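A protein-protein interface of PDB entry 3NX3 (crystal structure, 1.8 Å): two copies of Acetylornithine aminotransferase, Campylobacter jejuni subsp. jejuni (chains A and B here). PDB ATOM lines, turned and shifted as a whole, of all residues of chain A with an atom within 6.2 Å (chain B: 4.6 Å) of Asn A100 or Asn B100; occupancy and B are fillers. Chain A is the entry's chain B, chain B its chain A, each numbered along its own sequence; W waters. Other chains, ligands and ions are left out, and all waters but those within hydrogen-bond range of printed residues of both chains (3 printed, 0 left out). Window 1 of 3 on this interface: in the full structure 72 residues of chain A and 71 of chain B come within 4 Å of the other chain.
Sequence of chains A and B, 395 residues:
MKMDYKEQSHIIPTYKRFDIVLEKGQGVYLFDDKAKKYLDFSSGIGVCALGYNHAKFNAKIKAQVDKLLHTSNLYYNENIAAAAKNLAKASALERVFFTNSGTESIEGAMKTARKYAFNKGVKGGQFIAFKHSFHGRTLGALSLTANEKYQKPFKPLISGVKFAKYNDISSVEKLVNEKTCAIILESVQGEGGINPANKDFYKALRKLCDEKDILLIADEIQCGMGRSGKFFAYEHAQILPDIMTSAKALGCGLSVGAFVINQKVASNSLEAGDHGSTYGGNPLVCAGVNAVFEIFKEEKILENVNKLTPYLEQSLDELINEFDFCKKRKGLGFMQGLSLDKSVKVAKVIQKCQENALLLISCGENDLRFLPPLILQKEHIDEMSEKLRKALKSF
Asn B100 touches its own counterpart, Asn A100. Asn A100 touches Ser B101, and with the chains exchanged Ser A101 touches Asn B100. Asn A100 touches Ser B255, and with the chains exchanged Ser A255 touches Asn B100. Ser A101 touches Glu B104, and with the chains exchanged Glu A104 touches Ser B101. Positions printed for both chains: 99, 100, 101, 104, 255, 256 and 257. Of the 10 pairs that touch across the chains among the printed residues, 8 have their exchanged pair printed and touching as well.
The side-chain carboxylate (OE1) of Glu A104 sits at hydrogen-bond distance from the backbone NH (N) of Asn A100 (3.0 Å). N of Asn B100 lies within hydrogen-bond range of OE1 of Glu B104, 2.9 Å away. OG1 of Thr B99 sits at hydrogen-bond distance from O of Ser B101 (3.0 Å). O of Ser A101 is in hydrogen-bond range of OG1 of Thr A99 (2.9 Å). The side-chain hydroxyl (OG) of Ser A101 is in hydrogen-bond range of the backbone NH (N) of Glu A104 (3.1 Å). The side-chain hydroxyl of Ser A105 is in hydrogen-bond range of the backbone carbonyl oxygen of Ser A101.
Of the 13 printed residues of chain A, 6 touch a printed residue of chain B. Among the printed residues, 10 pairs touch across the chains. Among the printed residues, no Asp or Glu carboxylate lies within 4 Å of a Lys or Arg side-chain nitrogen of the other chain.
Among the printed residues, pairs that only touch across the chains: Asn A100 with Asn B100 (3.7 Å), Asn A100 with Ser B101 (3.6 Å), Ser A101 with Asn B100 (3.6 Å), Thr A103 with Glu B104 (3.7 Å) and Asn A282 with Ser B255 (3.5 Å).
Asn A100 touches just these residues of chain B: Asn B100 (3.7 Å), Ser B101 (3.6 Å) and Ser B255 (3.2 Å). Printed residues of chain B within 4 Å of Ser A101: Asn B100 (3.6 Å) and Glu B104 (2.4 Å). Of chain A, only Asn A100, Ser A101 and Ser A255 come within 4 Å of Asn B100. Printed residues of chain A within 4 Å of Ser B101: Asn A100 and Glu A104.
Water W3 lies within hydrogen-bond range of the side-chain hydroxyl of Ser A255 (2.4 Å), the backbone carbonyl oxygen of Ser B255 (2.7 Å) and the side-chain amide oxygen of Asn B100 (2.8 Å). Water W2 lies within hydrogen-bond range of the side-chain hydroxyl (OG) of Ser B255, the backbone carbonyl oxygen (O) of Ser A255, the side-chain amide oxygen (OD1) of Asn A100 and the side-chain amide nitrogen (ND2) of Asn A282. Water W1 lies within hydrogen-bond range of the side-chain hydroxyl (OG) of Ser B255 (2.7 Å) and the side-chain amide oxygen (OD1) of Asn A100 (2.8 Å).
The side-chain carboxylate of Glu B104 sits close to the side-chain carboxylate of Glu A104. The side-chain hydroxyl (OG) of Ser B101 lies within hydrogen-bond range of the side-chain carboxylate (OE2) of Glu A104. OG of Ser B255 sits at hydrogen-bond distance from OD1 of Asn A100 (3.2 Å). The side-chain amide oxygen (OD1) of Asn B100 lies within hydrogen-bond range of the side-chain hydroxyl (OG) of Ser A255. OE2 of Glu B104 is in hydrogen-bond range of OG of Ser A101, at 2.4 Å.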
ATOM      1  N   PHE A  98      -7.772  12.414  18.946  1.00  0.00           N
ATOM      2  CA  PHE A  98      -6.914  12.541  17.765  1.00  0.00           C
ATOM      3  C   PHE A  98      -6.648  14.000  17.402  1.00  0.00           C
ATOM      4  O   PHE A  98      -7.511  14.870  17.580  1.00  0.00           O
ATOM      5  CB  PHE A  98      -7.502  11.785  16.565  1.00  0.00           C
ATOM      6  CG  PHE A  98      -7.485  10.287  16.722  1.00  0.00           C
ATOM      7  CD1 PHE A  98      -6.288   9.586  16.653  1.00  0.00           C
ATOM      8  CD2 PHE A  98      -8.662   9.573  16.917  1.00  0.00           C
ATOM      9  CE1 PHE A  98      -6.254   8.219  16.808  1.00  0.00           C
ATOM     10  CE2 PHE A  98      -8.633   8.193  17.058  1.00  0.00           C
ATOM     11  CZ  PHE A  98      -7.426   7.517  17.001  1.00  0.00           C
ATOM     12  N   THR A  99      -5.446  14.251  16.895  1.00  0.00           N
ATOM     13  CA  THR A  99      -5.040  15.573  16.440  1.00  0.00           C
ATOM     14  C   THR A  99      -4.370  15.384  15.082  1.00  0.00           C
ATOM     15  O   THR A  99      -4.334  14.274  14.556  1.00  0.00           O
ATOM     16  CB  THR A  99      -3.995  16.206  17.374  1.00  0.00           C
ATOM     17  OG1 THR A  99      -2.788  15.438  17.294  1.00  0.00           O
ATOM     18  CG2 THR A  99      -4.491  16.258  18.838  1.00  0.00           C
ATOM     19  N   ASN A 100      -3.828  16.463  14.517  1.00  0.00           N
ATOM     20  CA  ASN A 100      -3.160  16.379  13.219  1.00  0.00           C
ATOM     21  C   ASN A 100      -1.656  16.179  13.315  1.00  0.00           C
ATOM     22  O   ASN A 100      -0.988  15.976  12.305  1.00  0.00           O
ATOM     23  CB  ASN A 100      -3.449  17.625  12.377  1.00  0.00           C
ATOM     24  CG  ASN A 100      -4.933  17.834  12.154  1.00  0.00           C
ATOM     25  OD1 ASN A 100      -5.582  17.036  11.482  1.00  0.00           O
ATOM     26  ND2 ASN A 100      -5.480  18.893  12.740  1.00  0.00           N
ATOM     27  N   SER A 101      -1.113  16.218  14.526  1.00  0.00           N
ATOM     28  CA  SER A 101       0.329  16.190  14.654  1.00  0.00           C
ATOM     29  C   SER A 101       0.796  15.941  16.069  1.00  0.00           C
ATOM     30  O   SER A 101       0.024  16.079  17.018  1.00  0.00           O
ATOM     31  CB  SER A 101       0.922  17.519  14.178  1.00  0.00           C
ATOM     32  OG  SER A 101       0.602  18.566  15.083  1.00  0.00           O
ATOM     33  N   GLY A 102       2.081  15.616  16.189  1.00  0.00           N
ATOM     34  CA  GLY A 102       2.727  15.435  17.475  1.00  0.00           C
ATOM     35  C   GLY A 102       2.625  16.690  18.317  1.00  0.00           C
ATOM     36  O   GLY A 102       2.227  16.637  19.479  1.00  0.00           O
ATOM     37  N   THR A 103       2.971  17.836  17.738  1.00  0.00           N
ATOM     38  CA  THR A 103       2.936  19.062  18.525  1.00  0.00           C
ATOM     39  C   THR A 103       1.509  19.421  18.966  1.00  0.00           C
ATOM     40  O   THR A 103       1.304  19.896  20.076  1.00  0.00           O
ATOM     41  CB  THR A 103       3.628  20.225  17.794  1.00  0.00           C
ATOM     42  OG1 THR A 103       3.881  21.291  18.726  1.00  0.00           O
ATOM     43  CG2 THR A 103       2.762  20.719  16.613  1.00  0.00           C
ATOM     44  N   GLU A 104       0.509  19.171  18.121  1.00  0.00           N
ATOM     45  CA  GLU A 104      -0.868  19.387  18.565  1.00  0.00           C
ATOM     46  C   GLU A 104      -1.262  18.480  19.723  1.00  0.00           C
ATOM     47  O   GLU A 104      -2.026  18.892  20.607  1.00  0.00           O
ATOM     48  CB  GLU A 104      -1.859  19.207  17.421  1.00  0.00           C
ATOM     49  CG  GLU A 104      -1.955  20.362  16.474  1.00  0.00           C
ATOM     50  CD  GLU A 104      -2.773  19.982  15.255  1.00  0.00           C
ATOM     51  OE1 GLU A 104      -3.830  19.334  15.442  1.00  0.00           O
ATOM     52  OE2 GLU A 104      -2.329  20.282  14.121  1.00  0.00           O
ATOM     53  N   SER A 105      -0.745  17.248  19.727  1.00  0.00           N
ATOM     54  CA  SER A 105      -1.024  16.308  20.817  1.00  0.00           C
ATOM     55  C   SER A 105      -0.439  16.774  22.146  1.00  0.00           C
ATOM     56  O   SER A 105      -1.066  16.626  23.197  1.00  0.00           O
ATOM     57  CB  SER A 105      -0.478  14.917  20.486  1.00  0.00           C
ATOM     58  OG  SER A 105      -1.058  14.445  19.283  1.00  0.00           O
ATOM     59  N   SER A 255      -0.535  12.205   8.299  1.00  0.00           N
ATOM     60  CA  SER A 255      -0.480  13.210   9.365  1.00  0.00           C
ATOM     61  C   SER A 255      -1.529  12.958  10.438  1.00  0.00           C
ATOM     62  O   SER A 255      -2.694  13.261  10.231  1.00  0.00           O
ATOM     63  CB  SER A 255      -0.746  14.598   8.775  1.00  0.00           C
ATOM     64  OG  SER A 255       0.202  14.921   7.776  1.00  0.00           O
ATOM     65  N   VAL A 256      -1.116  12.437  11.591  1.00  0.00           N
ATOM     66  CA  VAL A 256      -2.053  12.205  12.671  1.00  0.00           C
ATOM     67  C   VAL A 256      -1.284  12.165  13.983  1.00  0.00           C
ATOM     68  O   VAL A 256      -0.122  11.748  14.012  1.00  0.00           O
ATOM     69  CB  VAL A 256      -2.847  10.881  12.466  1.00  0.00           C
ATOM     70  CG1 VAL A 256      -1.919   9.667  12.506  1.00  0.00           C
ATOM     71  CG2 VAL A 256      -3.950  10.748  13.515  1.00  0.00           C
ATOM     72  N   GLY A 257      -1.948  12.595  15.044  1.00  0.00           N
ATOM     73  CA  GLY A 257      -1.394  12.616  16.378  1.00  0.00           C
ATOM     74  C   GLY A 257      -2.504  12.294  17.355  1.00  0.00           C
ATOM     75  O   GLY A 257      -3.676  12.323  16.995  1.00  0.00           O
ATOM     76  N   GLY A 281      -9.333  14.181  14.441  1.00  0.00           N
ATOM     77  CA  GLY A 281      -9.255  12.936  13.691  1.00  0.00           C
ATOM     78  C   GLY A 281     -10.082  13.068  12.427  1.00  0.00           C
ATOM     79  O   GLY A 281     -10.925  13.960  12.333  1.00  0.00           O
ATOM     80  N   ASN A 282      -9.834  12.210  11.445  1.00  0.00           N
ATOM     81  CA  ASN A 282     -10.687  12.166  10.259  1.00  0.00           C
ATOM     82  C   ASN A 282     -10.716  10.734   9.742  1.00  0.00           C
ATOM     83  O   ASN A 282      -9.887   9.924  10.141  1.00  0.00           O
ATOM     84  CB  ASN A 282     -10.217  13.151   9.187  1.00  0.00           C
ATOM     85  CG  ASN A 282      -8.805  12.876   8.725  1.00  0.00           C
ATOM     86  OD1 ASN A 282      -8.566  11.953   7.950  1.00  0.00           O
ATOM     87  ND2 ASN A 282      -7.859  13.675   9.202  1.00  0.00           N
ATOM     88  N   THR B  99       2.095  23.477   7.017  1.00  0.00           N
ATOM     89  CA  THR B  99       1.915  22.921   8.352  1.00  0.00           C
ATOM     90  C   THR B  99       0.875  21.822   8.208  1.00  0.00           C
ATOM     91  O   THR B  99       0.432  21.545   7.088  1.00  0.00           O
ATOM     92  CB  THR B  99       1.347  23.971   9.306  1.00  0.00           C
ATOM     93  OG1 THR B  99       0.043  24.338   8.850  1.00  0.00           O
ATOM     94  CG2 THR B  99       2.253  25.218   9.309  1.00  0.00           C
ATOM     95  N   ASN B 100       0.454  21.232   9.328  1.00  0.00           N
ATOM     96  CA  ASN B 100      -0.563  20.175   9.296  1.00  0.00           C
ATOM     97  C   ASN B 100      -1.993  20.639   9.562  1.00  0.00           C
ATOM     98  O   ASN B 100      -2.932  19.837   9.509  1.00  0.00           O
ATOM     99  CB  ASN B 100      -0.227  19.094  10.314  1.00  0.00           C
ATOM    100  CG  ASN B 100       1.145  18.536  10.109  1.00  0.00           C
ATOM    101  OD1 ASN B 100       1.392  17.832   9.131  1.00  0.00           O
ATOM    102  ND2 ASN B 100       2.059  18.869  11.007  1.00  0.00           N
ATOM    103  N   SER B 101      -2.167  21.917   9.862  1.00  0.00           N
ATOM    104  CA  SER B 101      -3.480  22.393  10.268  1.00  0.00           C
ATOM    105  C   SER B 101      -3.553  23.909  10.326  1.00  0.00           C
ATOM    106  O   SER B 101      -2.525  24.601  10.288  1.00  0.00           O
ATOM    107  CB  SER B 101      -3.822  21.842  11.656  1.00  0.00           C
ATOM    108  OG  SER B 101      -2.975  22.438  12.642  1.00  0.00           O
ATOM    109  N   GLU B 104      -1.871  25.302  13.530  1.00  0.00           N
ATOM    110  CA  GLU B 104      -0.409  25.299  13.443  1.00  0.00           C
ATOM    111  C   GLU B 104       0.057  26.461  12.586  1.00  0.00           C
ATOM    112  O   GLU B 104       1.114  27.035  12.837  1.00  0.00           O
ATOM    113  CB  GLU B 104       0.129  24.005  12.827  1.00  0.00           C
ATOM    114  CG  GLU B 104       0.241  22.842  13.772  1.00  0.00           C
ATOM    115  CD  GLU B 104       0.826  21.607  13.089  1.00  0.00           C
ATOM    116  OE1 GLU B 104       1.475  21.734  12.019  1.00  0.00           O
ATOM    117  OE2 GLU B 104       0.624  20.506  13.623  1.00  0.00           O
ATOM    118  N   SER B 255      -5.242  16.800   5.630  1.00  0.00           N
ATOM    119  CA  SER B 255      -4.731  17.646   6.714  1.00  0.00           C
ATOM    120  C   SER B 255      -3.542  18.514   6.302  1.00  0.00           C
ATOM    121  O   SER B 255      -2.398  18.072   6.339  1.00  0.00           O
ATOM    122  CB  SER B 255      -4.302  16.762   7.889  1.00  0.00           C
ATOM    123  OG  SER B 255      -5.425  16.093   8.429  1.00  0.00           O
ATOM    124  N   VAL B 256      -3.804  19.767   5.968  1.00  0.00           N
ATOM    125  CA  VAL B 256      -2.699  20.630   5.575  1.00  0.00           C
ATOM    126  C   VAL B 256      -3.050  22.059   5.875  1.00  0.00           C
ATOM    127  O   VAL B 256      -4.220  22.444   5.822  1.00  0.00           O
ATOM    128  CB  VAL B 256      -2.304  20.448   4.077  1.00  0.00           C
ATOM    129  CG1 VAL B 256      -3.479  20.739   3.174  1.00  0.00           C
ATOM    130  CG2 VAL B 256      -1.104  21.355   3.709  1.00  0.00           C
ATOM    131  N   GLY B 257      -2.037  22.841   6.196  1.00  0.00           N
ATOM    132  CA  GLY B 257      -2.209  24.236   6.516  1.00  0.00           C
ATOM    133  C   GLY B 257      -0.971  24.973   6.076  1.00  0.00           C
ATOM    134  O   GLY B 257       0.048  24.359   5.783  1.00  0.00           O
HETATM  135  O   HOH W   1      -7.301  17.720   9.443  1.00  0.00           O
HETATM  136  O   HOH W   2      -5.010  14.529  10.401  1.00  0.00           O
HETATM  137  O   HOH W   3       0.050  17.116   6.782  1.00  0.00           O
